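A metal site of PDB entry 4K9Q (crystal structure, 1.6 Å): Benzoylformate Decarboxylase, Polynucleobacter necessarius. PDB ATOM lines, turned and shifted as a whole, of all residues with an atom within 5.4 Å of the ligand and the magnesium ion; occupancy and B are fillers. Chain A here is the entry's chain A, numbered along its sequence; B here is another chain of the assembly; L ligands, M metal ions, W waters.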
ATOM      1  N   TYR A 278     -30.263   0.845  15.441  1.00  0.00           N
ATOM      2  CA  TYR A 278     -29.614   2.111  15.106  1.00  0.00           C
ATOM      3  C   TYR A 278     -30.625   3.269  15.110  1.00  0.00           C
ATOM      4  O   TYR A 278     -30.659   4.049  16.053  1.00  0.00           O
ATOM      5  CB  TYR A 278     -28.835   1.999  13.787  1.00  0.00           C
ATOM      6  CG  TYR A 278     -28.095   3.255  13.385  1.00  0.00           C
ATOM      7  CD1 TYR A 278     -27.769   4.230  14.319  1.00  0.00           C
ATOM      8  CD2 TYR A 278     -27.719   3.456  12.067  1.00  0.00           C
ATOM      9  CE1 TYR A 278     -27.104   5.389  13.944  1.00  0.00           C
ATOM     10  CE2 TYR A 278     -27.035   4.593  11.681  1.00  0.00           C
ATOM     11  CZ  TYR A 278     -26.735   5.559  12.629  1.00  0.00           C
ATOM     12  OH  TYR A 278     -26.050   6.706  12.245  1.00  0.00           O
ATOM     13  N   GLU A 372     -17.495   0.336   3.514  1.00  0.00           N
ATOM     14  CA  GLU A 372     -17.776   1.503   4.350  1.00  0.00           C
ATOM     15  C   GLU A 372     -18.328   2.578   3.432  1.00  0.00           C
ATOM     16  O   GLU A 372     -17.677   3.574   3.136  1.00  0.00           O
ATOM     17  CB  GLU A 372     -16.509   1.985   5.067  1.00  0.00           C
ATOM     18  CG  GLU A 372     -16.766   3.024   6.162  1.00  0.00           C
ATOM     19  CD  GLU A 372     -15.519   3.367   6.951  1.00  0.00           C
ATOM     20  OE1 GLU A 372     -15.021   2.514   7.715  1.00  0.00           O
ATOM     21  OE2 GLU A 372     -15.018   4.502   6.787  1.00  0.00           O
ATOM     22  N   CYS A 373     -19.547   2.324   2.949  1.00  0.00           N
ATOM     23  CA  CYS A 373     -20.259   3.241   2.060  1.00  0.00           C
ATOM     24  C   CYS A 373     -21.699   3.134   2.508  1.00  0.00           C
ATOM     25  O   CYS A 373     -22.487   2.375   1.939  1.00  0.00           O
ATOM     26  CB  CYS A 373     -20.103   2.791   0.605  1.00  0.00           C
ATOM     27  SG  CYS A 373     -20.684   4.024  -0.567  1.00  0.00           S
ATOM     28  N   PRO A 374     -22.050   3.875   3.565  1.00  0.00           N
ATOM     29  CA  PRO A 374     -23.307   3.606   4.269  1.00  0.00           C
ATOM     30  C   PRO A 374     -24.567   3.614   3.413  1.00  0.00           C
ATOM     31  O   PRO A 374     -25.404   2.710   3.575  1.00  0.00           O
ATOM     32  CB  PRO A 374     -23.345   4.725   5.322  1.00  0.00           C
ATOM     33  CG  PRO A 374     -21.889   4.946   5.651  1.00  0.00           C
ATOM     34  CD  PRO A 374     -21.188   4.824   4.293  1.00  0.00           C
ATOM     35  N   SER A 375     -24.719   4.571   2.504  1.00  0.00           N
ATOM     36  CA  SER A 375     -25.994   4.665   1.777  1.00  0.00           C
ATOM     37  C   SER A 375     -26.268   3.484   0.844  1.00  0.00           C
ATOM     38  O   SER A 375     -27.420   3.226   0.509  1.00  0.00           O
ATOM     39  CB  SER A 375     -26.107   5.990   1.003  1.00  0.00           C
ATOM     40  OG  SER A 375     -25.255   5.996  -0.120  1.00  0.00           O
ATOM     41  N   ILE A 376     -25.232   2.740   0.440  1.00  0.00           N
ATOM     42  CA  ILE A 376     -25.424   1.644  -0.511  1.00  0.00           C
ATOM     43  C   ILE A 376     -25.537   0.246   0.107  1.00  0.00           C
ATOM     44  O   ILE A 376     -25.667  -0.750  -0.602  1.00  0.00           O
ATOM     45  CB  ILE A 376     -24.324   1.608  -1.622  1.00  0.00           C
ATOM     46  CG1 ILE A 376     -22.983   1.153  -1.039  1.00  0.00           C
ATOM     47  CG2 ILE A 376     -24.209   2.967  -2.300  1.00  0.00           C
ATOM     48  CD1 ILE A 376     -21.892   0.961  -2.100  1.00  0.00           C
ATOM     49  N   GLY A 398     -19.786   1.192  13.586  1.00  0.00           N
ATOM     50  CA  GLY A 398     -20.256   2.342  12.826  1.00  0.00           C
ATOM     51  C   GLY A 398     -19.301   3.530  12.789  1.00  0.00           C
ATOM     52  O   GLY A 398     -19.649   4.580  12.232  1.00  0.00           O
ATOM     53  N   GLY A 399     -18.114   3.390  13.373  1.00  0.00           N
ATOM     54  CA  GLY A 399     -17.128   4.459  13.380  1.00  0.00           C
ATOM     55  C   GLY A 399     -16.346   4.591  12.080  1.00  0.00           C
ATOM     56  O   GLY A 399     -15.465   3.783  11.787  1.00  0.00           O
ATOM     57  N   LEU A 400     -16.663   5.615  11.306  1.00  0.00           N
ATOM     58  CA  LEU A 400     -16.005   5.814  10.026  1.00  0.00           C
ATOM     59  C   LEU A 400     -14.502   6.034  10.197  1.00  0.00           C
ATOM     60  O   LEU A 400     -14.050   6.574  11.214  1.00  0.00           O
ATOM     61  CB  LEU A 400     -16.626   7.004   9.285  1.00  0.00           C
ATOM     62  CG  LEU A 400     -18.121   6.882   9.000  1.00  0.00           C
ATOM     63  CD1 LEU A 400     -18.602   8.120   8.224  1.00  0.00           C
ATOM     64  CD2 LEU A 400     -18.395   5.607   8.203  1.00  0.00           C
ATOM     65  N   GLY A 428     -17.505   5.068   0.622  1.00  0.00           N
ATOM     66  CA  GLY A 428     -18.152   6.335   0.318  1.00  0.00           C
ATOM     67  C   GLY A 428     -17.110   7.441   0.220  1.00  0.00           C
ATOM     68  O   GLY A 428     -16.011   7.319   0.789  1.00  0.00           O
ATOM     69  N   ASP A 429     -17.429   8.520  -0.481  1.00  0.00           N
ATOM     70  CA  ASP A 429     -16.487   9.634  -0.588  1.00  0.00           C
ATOM     71  C   ASP A 429     -16.229  10.355   0.758  1.00  0.00           C
ATOM     72  O   ASP A 429     -15.109  10.767   1.035  1.00  0.00           O
ATOM     73  CB  ASP A 429     -16.823  10.613  -1.730  1.00  0.00           C
ATOM     74  CG  ASP A 429     -18.243  11.158  -1.676  1.00  0.00           C
ATOM     75  OD1 ASP A 429     -19.085  10.593  -0.967  1.00  0.00           O
ATOM     76  OD2 ASP A 429     -18.526  12.152  -2.386  1.00  0.00           O
ATOM     77  N   GLY A 430     -17.280  10.494   1.578  1.00  0.00           N
ATOM     78  CA  GLY A 430     -17.120  11.035   2.919  1.00  0.00           C
ATOM     79  C   GLY A 430     -16.294  10.120   3.812  1.00  0.00           C
ATOM     80  O   GLY A 430     -15.337  10.552   4.464  1.00  0.00           O
ATOM     81  N   SER A 431     -16.678   8.842   3.846  1.00  0.00           N
ATOM     82  CA  SER A 431     -15.979   7.843   4.653  1.00  0.00           C
ATOM     83  C   SER A 431     -14.501   7.762   4.310  1.00  0.00           C
ATOM     84  O   SER A 431     -13.666   7.618   5.194  1.00  0.00           O
ATOM     85  CB  SER A 431     -16.614   6.452   4.455  1.00  0.00           C
ATOM     86  OG  SER A 431     -17.896   6.379   5.048  1.00  0.00           O
ATOM     87  N   PHE A 432     -14.194   7.844   3.015  1.00  0.00           N
ATOM     88  CA  PHE A 432     -12.823   7.758   2.503  1.00  0.00           C
ATOM     89  C   PHE A 432     -11.872   8.755   3.186  1.00  0.00           C
ATOM     90  O   PHE A 432     -10.689   8.463   3.363  1.00  0.00           O
ATOM     91  CB  PHE A 432     -12.855   8.029   0.989  1.00  0.00           C
ATOM     92  CG  PHE A 432     -11.615   7.595   0.232  1.00  0.00           C
ATOM     93  CD1 PHE A 432     -11.398   6.257  -0.058  1.00  0.00           C
ATOM     94  CD2 PHE A 432     -10.728   8.535  -0.245  1.00  0.00           C
ATOM     95  CE1 PHE A 432     -10.278   5.868  -0.789  1.00  0.00           C
ATOM     96  CE2 PHE A 432      -9.614   8.159  -0.985  1.00  0.00           C
ATOM     97  CZ  PHE A 432      -9.392   6.822  -1.242  1.00  0.00           C
ATOM     98  N   TYR A 434     -11.749   9.981   6.358  1.00  0.00           N
ATOM     99  CA  TYR A 434     -11.398   9.932   7.775  1.00  0.00           C
ATOM    100  C   TYR A 434      -9.997   9.392   8.021  1.00  0.00           C
ATOM    101  O   TYR A 434      -9.247   9.946   8.821  1.00  0.00           O
ATOM    102  CB  TYR A 434     -12.419   9.130   8.597  1.00  0.00           C
ATOM    103  CG  TYR A 434     -13.752   9.854   8.716  1.00  0.00           C
ATOM    104  CD1 TYR A 434     -14.697   9.799   7.695  1.00  0.00           C
ATOM    105  CD2 TYR A 434     -14.072  10.578   9.870  1.00  0.00           C
ATOM    106  CE1 TYR A 434     -15.895  10.464   7.799  1.00  0.00           C
ATOM    107  CE2 TYR A 434     -15.281  11.242   9.982  1.00  0.00           C
ATOM    108  CZ  TYR A 434     -16.193  11.185   8.946  1.00  0.00           C
ATOM    109  OH  TYR A 434     -17.399  11.829   9.013  1.00  0.00           O
ATOM    110  N   PHE A 454     -17.479   5.496  -4.181  1.00  0.00           N
ATOM    111  CA  PHE A 454     -18.778   5.923  -4.678  1.00  0.00           C
ATOM    112  C   PHE A 454     -18.973   7.408  -4.405  1.00  0.00           C
ATOM    113  O   PHE A 454     -19.285   7.818  -3.293  1.00  0.00           O
ATOM    114  CB  PHE A 454     -19.889   5.093  -4.027  1.00  0.00           C
ATOM    115  CG  PHE A 454     -19.895   3.649  -4.469  1.00  0.00           C
ATOM    116  CD1 PHE A 454     -18.880   2.784  -4.089  1.00  0.00           C
ATOM    117  CD2 PHE A 454     -20.908   3.170  -5.278  1.00  0.00           C
ATOM    118  CE1 PHE A 454     -18.885   1.462  -4.516  1.00  0.00           C
ATOM    119  CE2 PHE A 454     -20.924   1.847  -5.697  1.00  0.00           C
ATOM    120  CZ  PHE A 454     -19.910   0.982  -5.317  1.00  0.00           C
ATOM    121  N   ASN A 456     -20.863  10.599  -4.452  1.00  0.00           N
ATOM    122  CA  ASN A 456     -22.105  11.367  -4.576  1.00  0.00           C
ATOM    123  C   ASN A 456     -21.983  12.801  -4.039  1.00  0.00           C
ATOM    124  O   ASN A 456     -22.960  13.547  -3.987  1.00  0.00           O
ATOM    125  CB  ASN A 456     -23.307  10.638  -3.944  1.00  0.00           C
ATOM    126  CG  ASN A 456     -23.077  10.268  -2.492  1.00  0.00           C
ATOM    127  OD1 ASN A 456     -22.120  10.711  -1.889  1.00  0.00           O
ATOM    128  ND2 ASN A 456     -23.967   9.451  -1.917  1.00  0.00           N
ATOM    129  N   GLU A 457     -20.757  13.187  -3.683  1.00  0.00           N
ATOM    130  CA  GLU A 457     -20.444  14.524  -3.168  1.00  0.00           C
ATOM    131  C   GLU A 457     -21.290  14.925  -1.971  1.00  0.00           C
ATOM    132  O   GLU A 457     -21.641  16.098  -1.816  1.00  0.00           O
ATOM    133  CB  GLU A 457     -20.554  15.566  -4.291  1.00  0.00           C
ATOM    134  CG  GLU A 457     -19.676  15.196  -5.465  1.00  0.00           C
ATOM    135  CD  GLU A 457     -19.472  16.323  -6.453  1.00  0.00           C
ATOM    136  OE1 GLU A 457     -20.479  16.870  -6.947  1.00  0.00           O
ATOM    137  OE2 GLU A 457     -18.302  16.671  -6.731  1.00  0.00           O
ATOM    138  N   GLU A 458     -21.604  13.962  -1.119  1.00  0.00           N
ATOM    139  CA  GLU A 458     -22.422  14.227   0.067  1.00  0.00           C
ATOM    140  C   GLU A 458     -22.256  13.149   1.121  1.00  0.00           C
ATOM    141  O   GLU A 458     -21.782  12.054   0.820  1.00  0.00           O
ATOM    142  CB  GLU A 458     -23.908  14.310  -0.341  1.00  0.00           C
ATOM    143  CG  GLU A 458     -24.477  12.963  -0.818  1.00  0.00           C
ATOM    144  CD  GLU A 458     -25.814  13.084  -1.573  1.00  0.00           C
ATOM    145  OE1 GLU A 458     -26.414  14.177  -1.569  1.00  0.00           O
ATOM    146  OE2 GLU A 458     -26.238  12.064  -2.161  1.00  0.00           O
ATOM    147  N   TYR A 459     -22.632  13.447   2.354  1.00  0.00           N
ATOM    148  CA  TYR A 459     -22.798  12.424   3.361  1.00  0.00           C
ATOM    149  C   TYR A 459     -24.218  11.873   3.170  1.00  0.00           C
ATOM    150  O   TYR A 459     -25.157  12.263   3.866  1.00  0.00           O
ATOM    151  CB  TYR A 459     -22.644  13.026   4.755  1.00  0.00           C
ATOM    152  CG  TYR A 459     -21.233  13.426   5.194  1.00  0.00           C
ATOM    153  CD1 TYR A 459     -20.122  12.582   5.025  1.00  0.00           C
ATOM    154  CD2 TYR A 459     -21.018  14.642   5.841  1.00  0.00           C
ATOM    155  CE1 TYR A 459     -18.853  12.951   5.469  1.00  0.00           C
ATOM    156  CE2 TYR A 459     -19.758  15.013   6.284  1.00  0.00           C
ATOM    157  CZ  TYR A 459     -18.687  14.168   6.106  1.00  0.00           C
ATOM    158  OH  TYR A 459     -17.436  14.558   6.562  1.00  0.00           O
ATOM    159  N   GLY A 460     -24.381  10.991   2.175  1.00  0.00           N
ATOM    160  CA  GLY A 460     -25.691  10.568   1.721  1.00  0.00           C
ATOM    161  C   GLY A 460     -26.602  10.019   2.805  1.00  0.00           C
ATOM    162  O   GLY A 460     -27.774  10.399   2.908  1.00  0.00           O
ATOM    163  N   ILE A 461     -26.070   9.110   3.606  1.00  0.00           N
ATOM    164  CA  ILE A 461     -26.924   8.452   4.585  1.00  0.00           C
ATOM    165  C   ILE A 461     -27.412   9.443   5.643  1.00  0.00           C
ATOM    166  O   ILE A 461     -28.476   9.248   6.215  1.00  0.00           O
ATOM    167  CB  ILE A 461     -26.252   7.227   5.225  1.00  0.00           C
ATOM    168  CG1 ILE A 461     -27.323   6.379   5.922  1.00  0.00           C
ATOM    169  CG2 ILE A 461     -25.182   7.659   6.193  1.00  0.00           C
ATOM    170  CD1 ILE A 461     -26.845   5.034   6.405  1.00  0.00           C
ATOM    171  N   LEU A 462     -26.651  10.513   5.885  1.00  0.00           N
ATOM    172  CA  LEU A 462     -27.143  11.534   6.824  1.00  0.00           C
ATOM    173  C   LEU A 462     -28.357  12.285   6.265  1.00  0.00           C
ATOM    174  O   LEU A 462     -29.208  12.759   7.028  1.00  0.00           O
ATOM    175  CB  LEU A 462     -26.047  12.511   7.231  1.00  0.00           C
ATOM    176  CG  LEU A 462     -24.843  11.907   7.964  1.00  0.00           C
ATOM    177  CD1 LEU A 462     -23.888  12.997   8.427  1.00  0.00           C
ATOM    178  CD2 LEU A 462     -25.287  11.025   9.129  1.00  0.00           C
ATOM    179  N   LEU A 479     -20.450  17.650   0.187  1.00  0.00           N
ATOM    180  CA  LEU A 479     -19.005  17.526   0.047  1.00  0.00           C
ATOM    181  C   LEU A 479     -18.495  17.922  -1.349  1.00  0.00           C
ATOM    182  O   LEU A 479     -17.888  17.107  -2.045  1.00  0.00           O
ATOM    183  CB  LEU A 479     -18.572  16.092   0.324  1.00  0.00           C
ATOM    184  CG  LEU A 479     -18.896  15.525   1.704  1.00  0.00           C
ATOM    185  CD1 LEU A 479     -18.544  14.036   1.786  1.00  0.00           C
ATOM    186  CD2 LEU A 479     -18.185  16.338   2.799  1.00  0.00           C
ATOM    187  N   LEU A 528     -31.009   9.551  -3.368  1.00  0.00           N
ATOM    188  CA  LEU A 528     -30.846   8.541  -2.331  1.00  0.00           C
ATOM    189  C   LEU A 528     -32.141   7.786  -2.099  1.00  0.00           C
ATOM    190  O   LEU A 528     -33.217   8.382  -2.005  1.00  0.00           O
ATOM    191  CB  LEU A 528     -30.399   9.199  -1.020  1.00  0.00           C
ATOM    192  CG  LEU A 528     -29.025   9.891  -0.999  1.00  0.00           C
ATOM    193  CD1 LEU A 528     -28.994  10.961   0.080  1.00  0.00           C
ATOM    194  CD2 LEU A 528     -27.907   8.856  -0.757  1.00  0.00           C
ATOM    195  N   ASN B  23     -18.269  17.743  12.808  1.00  0.00           N
ATOM    196  CA  ASN B  23     -18.420  16.732  11.779  1.00  0.00           C
ATOM    197  C   ASN B  23     -19.679  15.977  12.164  1.00  0.00           C
ATOM    198  O   ASN B  23     -19.734  15.366  13.247  1.00  0.00           O
ATOM    199  CB  ASN B  23     -17.197  15.823  11.724  1.00  0.00           C
ATOM    200  CG  ASN B  23     -17.346  14.718  10.696  1.00  0.00           C
ATOM    201  OD1 ASN B  23     -17.719  13.587  11.023  1.00  0.00           O
ATOM    202  ND2 ASN B  23     -17.061  15.034   9.435  1.00  0.00           N
ATOM    203  N   PRO B  24     -20.730  16.062  11.326  1.00  0.00           N
ATOM    204  CA  PRO B  24     -22.057  15.628  11.763  1.00  0.00           C
ATOM    205  C   PRO B  24     -22.271  14.110  11.732  1.00  0.00           C
ATOM    206  O   PRO B  24     -21.562  13.393  11.035  1.00  0.00           O
ATOM    207  CB  PRO B  24     -22.988  16.320  10.741  1.00  0.00           C
ATOM    208  CG  PRO B  24     -22.164  16.400   9.502  1.00  0.00           C
ATOM    209  CD  PRO B  24     -20.756  16.665   9.985  1.00  0.00           C
ATOM    210  N   GLY B  25     -23.248  13.652  12.517  1.00  0.00           N
ATOM    211  CA  GLY B  25     -23.685  12.270  12.499  1.00  0.00           C
ATOM    212  C   GLY B  25     -25.165  12.245  12.851  1.00  0.00           C
ATOM    213  O   GLY B  25     -25.750  13.289  13.139  1.00  0.00           O
ATOM    214  N   SER B  26     -25.778  11.059  12.825  1.00  0.00           N
ATOM    215  CA  SER B  26     -27.218  10.949  13.023  1.00  0.00           C
ATOM    216  C   SER B  26     -27.645  11.464  14.382  1.00  0.00           C
ATOM    217  O   SER B  26     -28.716  12.069  14.522  1.00  0.00           O
ATOM    218  CB  SER B  26     -27.675   9.493  12.849  1.00  0.00           C
ATOM    219  OG  SER B  26     -27.175   8.678  13.891  1.00  0.00           O
ATOM    220  N   GLU B  47     -12.384  14.353  12.950  1.00  0.00           N
ATOM    221  CA  GLU B  47     -12.593  15.008  14.228  1.00  0.00           C
ATOM    222  C   GLU B  47     -11.355  15.611  14.891  1.00  0.00           C
ATOM    223  O   GLU B  47     -11.462  16.531  15.691  1.00  0.00           O
ATOM    224  CB  GLU B  47     -13.359  14.092  15.183  1.00  0.00           C
ATOM    225  CG  GLU B  47     -14.768  13.758  14.686  1.00  0.00           C
ATOM    226  CD  GLU B  47     -14.831  12.572  13.722  1.00  0.00           C
ATOM    227  OE1 GLU B  47     -13.775  12.087  13.261  1.00  0.00           O
ATOM    228  OE2 GLU B  47     -15.971  12.139  13.416  1.00  0.00           O
ATOM    229  N   HIS B  70     -19.605  13.220  16.638  1.00  0.00           N
ATOM    230  CA  HIS B  70     -20.567  12.129  16.580  1.00  0.00           C
ATOM    231  C   HIS B  70     -20.262  11.031  17.586  1.00  0.00           C
ATOM    232  O   HIS B  70     -19.452  10.153  17.326  1.00  0.00           O
ATOM    233  CB  HIS B  70     -20.595  11.529  15.181  1.00  0.00           C
ATOM    234  CG  HIS B  70     -21.543  10.374  15.028  1.00  0.00           C
ATOM    235  ND1 HIS B  70     -22.890  10.482  15.300  1.00  0.00           N
ATOM    236  CD2 HIS B  70     -21.336   9.103  14.635  1.00  0.00           C
ATOM    237  CE1 HIS B  70     -23.474   9.320  15.066  1.00  0.00           C
ATOM    238  NE2 HIS B  70     -22.559   8.473  14.647  1.00  0.00           N
ATOM    239  N   ALA B  73     -17.511   7.462  18.517  1.00  0.00           N
ATOM    240  CA  ALA B  73     -16.656   7.318  17.322  1.00  0.00           C
ATOM    241  C   ALA B  73     -15.934   8.624  17.031  1.00  0.00           C
ATOM    242  O   ALA B  73     -14.723   8.644  16.798  1.00  0.00           O
ATOM    243  CB  ALA B  73     -17.494   6.915  16.117  1.00  0.00           C
ATOM    244  N   GLY B  74     -16.699   9.705  17.018  1.00  0.00           N
ATOM    245  CA  GLY B  74     -16.165  11.025  16.753  1.00  0.00           C
ATOM    246  C   GLY B  74     -15.282  11.490  17.887  1.00  0.00           C
ATOM    247  O   GLY B  74     -14.187  12.024  17.662  1.00  0.00           O
ATOM    248  N   ASN B  77     -11.846   9.781  17.620  1.00  0.00           N
ATOM    249  CA  ASN B  77     -10.962  10.366  16.622  1.00  0.00           C
ATOM    250  C   ASN B  77     -10.363  11.691  17.080  1.00  0.00           C
ATOM    251  O   ASN B  77      -9.289  12.113  16.599  1.00  0.00           O
ATOM    252  CB  ASN B  77     -11.699  10.579  15.293  1.00  0.00           C
ATOM    253  CG  ASN B  77     -11.861   9.296  14.497  1.00  0.00           C
ATOM    254  OD1 ASN B  77     -11.275   8.270  14.838  1.00  0.00           O
ATOM    255  ND2 ASN B  77     -12.649   9.362  13.430  1.00  0.00           N
ATOM    256  N   LEU B 110     -23.724   2.739  18.120  1.00  0.00           N
ATOM    257  CA  LEU B 110     -23.304   4.138  18.254  1.00  0.00           C
ATOM    258  C   LEU B 110     -23.722   4.772  19.588  1.00  0.00           C
ATOM    259  O   LEU B 110     -23.800   6.002  19.718  1.00  0.00           O
ATOM    260  CB  LEU B 110     -23.718   4.964  17.023  1.00  0.00           C
ATOM    261  CG  LEU B 110     -22.870   4.601  15.793  1.00  0.00           C
ATOM    262  CD1 LEU B 110     -23.568   4.918  14.483  1.00  0.00           C
ATOM    263  CD2 LEU B 110     -21.494   5.275  15.843  1.00  0.00           C
HETATM  264  N1  LIG L   1     -17.700  10.471  12.267  1.00  0.00           N
HETATM  265  C1  LIG L   1     -17.301   9.177  12.545  1.00  0.00           C
HETATM  266  C2  LIG L   1     -15.906   8.905  13.021  1.00  0.00           C
HETATM  267  N2  LIG L   1     -18.172   8.110  12.406  1.00  0.00           N
HETATM  268  C3  LIG L   1     -19.458   8.344  11.977  1.00  0.00           C
HETATM  269  N3  LIG L   1     -20.304   7.319  11.862  1.00  0.00           N
HETATM  270  C4  LIG L   1     -19.862   9.636  11.666  1.00  0.00           C
HETATM  271  C5  LIG L   1     -18.994  10.708  11.826  1.00  0.00           C
HETATM  272  C6  LIG L   1     -21.284   9.888  11.202  1.00  0.00           C
HETATM  273  N4  LIG L   1     -21.625   9.428   9.860  1.00  0.00           N
HETATM  274  C7  LIG L   1     -22.334   8.276   9.581  1.00  0.00           C
HETATM  275  S1  LIG L   1     -22.605   8.025   8.014  1.00  0.00           S
HETATM  276  C8  LIG L   1     -21.844   9.399   7.631  1.00  0.00           C
HETATM  277  C9  LIG L   1     -21.340  10.110   8.725  1.00  0.00           C
HETATM  278  C10 LIG L   1     -20.584  11.410   8.658  1.00  0.00           C
HETATM  279  C11 LIG L   1     -21.798   9.748   6.170  1.00  0.00           C
HETATM  280  C12 LIG L   1     -21.060   8.759   5.289  1.00  0.00           C
HETATM  281  O1  LIG L   1     -20.919   9.406   4.044  1.00  0.00           O
HETATM  282  P1  LIG L   1     -20.262   8.667   2.770  1.00  0.00           P
HETATM  283  O2  LIG L   1     -19.067   7.891   3.226  1.00  0.00           O
HETATM  284  O3  LIG L   1     -19.898   9.668   1.727  1.00  0.00           O
HETATM  285  O4  LIG L   1     -21.358   7.579   2.350  1.00  0.00           O
HETATM  286  P2  LIG L   1     -22.783   7.816   1.643  1.00  0.00           P
HETATM  287  O5  LIG L   1     -23.804   7.822   2.743  1.00  0.00           O
HETATM  288  O6  LIG L   1     -22.997   6.634   0.722  1.00  0.00           O
HETATM  289  O7  LIG L   1     -22.824   9.120   0.910  1.00  0.00           O
HETATM  290 MG    MG M   1     -21.050  10.083  -0.085  1.00  0.00          MG
HETATM  291  O   HOH W   1     -20.762   7.946  -1.003  1.00  0.00           O
HETATM  292  O   HOH W   2     -22.931   6.985  12.401  1.00  0.00           O
HETATM  293  O   HOH W   3     -24.069   5.289   9.307  1.00  0.00           O
HETATM  294  O   HOH W   4     -22.151   4.839  10.887  1.00  0.00           O
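Merely in contact with the ligand: Tyr 434 (3.2 Å), Pro 24 of chain B (3.2 Å), Asn 77 of chain B (3.3 Å), His 70 of chain B (3.3 Å), Pro 374 (3.4 Å), Tyr 459 (3.4 Å), Gly 428 (3.4 Å), Gly 25 of chain B (3.6 Å), Leu 462 (3.7 Å), Gly 399 (3.9 Å) and Ala 73 of chain B (3.96 Å).
Hydrophobic or aromatic side chains within 4 Å of the ligand: Pro 374, Leu 400, Tyr 434, Tyr 459, Ile 461, Leu 462, His 70 of chain B and Ala 73 of chain B.
24 residues have an atom within 4 Å of the ligand: Cys 373, Pro 374, Ser 375, Gly 398, Gly 399, Leu 400, Gly 428, Asp 429, Gly 430, Ser 431, Tyr 434, Asn 456, Glu 458, Tyr 459, Gly 460, Ile 461, Leu 462, Asn 23 of chain B, Pro 24 of chain B, Gly 25 of chain B, Glu 47 of chain B, His 70 of chain B, Ala 73 of chain B and Asn 77 of chain B.
The backbone NH (N) of Ser 375 sits close to an oxygen (O6) of the ligand (3.2 Å).
An oxygen (O6) of the ligand sits at hydrogen-bond distance from the side-chain hydroxyl (OG) of Ser 375 (2.5 Å).
N of Ser 431 lies within hydrogen-bond range of O2 of the ligand, 2.6 Å away.
An oxygen (O2) of the ligand is in hydrogen-bond range of the side-chain hydroxyl (OG) of Ser 431, at 2.6 Å.
N1 of the ligand lies within hydrogen-bond range of OE2 of Glu 47 of chain B (2.7 Å).
An oxygen (O5) of the ligand is in hydrogen-bond range of the backbone NH (N) of Gly 460 (3.3 Å).
The backbone NH of Ile 461 is in hydrogen-bond range of an oxygen (O5) of the ligand (2.7 Å).
The backbone NH (N) of Gly 430 lies close to an oxygen (O3) of the ligand (2.7 Å).
N3 of the ligand lies within hydrogen-bond range of O of Gly 398 (2.8 Å).
The backbone NH (N) of Leu 400 is in hydrogen-bond range of a nitrogen (N2) of the ligand, 3.1 Å away.
OD1 of Asn 23 of chain B sits close to N1 of the ligand.
The side-chain sulfur of Cys 373 sits at hydrogen-bond distance from an oxygen (O6) of the ligand.
Water W1 lies within hydrogen-bond range of O of Phe 454 (2.7 Å), O6 of the ligand (3.1 Å) and N of Asp 429 (3.4 Å).
Water W2 lies within hydrogen-bond range of N3 of the ligand, NE2 of His 70 of chain B and OH of Tyr 278.
Water W4 bridges the backbone carbonyl oxygen of Gly 398 (2.9 Å) and a nitrogen (N3) of the ligand (3.2 Å).
Within 4 Å of the magnesium ion: Asp 429, Asn 456 and Glu 458.
N of Asp 429 lies within hydrogen-bond range of O of Phe 454 (3.4 Å).
The backbone carbonyl oxygen (O) of Glu 372 lies close to the side-chain hydroxyl (OG) of Ser 431, at 3.4 Å.
The side-chain carboxylate of Glu 47 of chain B sits close to the side-chain amide oxygen of Asn 23 of chain B (3.3 Å).
The side-chain amide nitrogen of Asn 77 of chain B lies within hydrogen-bond range of the side-chain carboxylate of Glu 47 of chain B (3.0 Å).
The side-chain hydroxyl (OH) of Tyr 434 is in hydrogen-bond range of the side-chain amide oxygen (OD1) of Asn 23 of chain B (2.7 Å).
OH of Tyr 459 lies within hydrogen-bond range of ND2 of Asn 23 of chain B (2.9 Å).
N of Gly 428 lies close to SG of Cys 373.
The backbone NH (N) of Gly 428 lies within hydrogen-bond range of the backbone carbonyl oxygen (O) of Glu 372, 2.9 Å away.
The magnesium ion is bound by O3 of the ligand (2.2 Å), OD1 of Asn 456 (2.2 Å), OD1 of Asp 429 (2.2 Å), O7 of the ligand (2.3 Å), O of Glu 458 (2.3 Å) and water W1 (2.3 Å).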
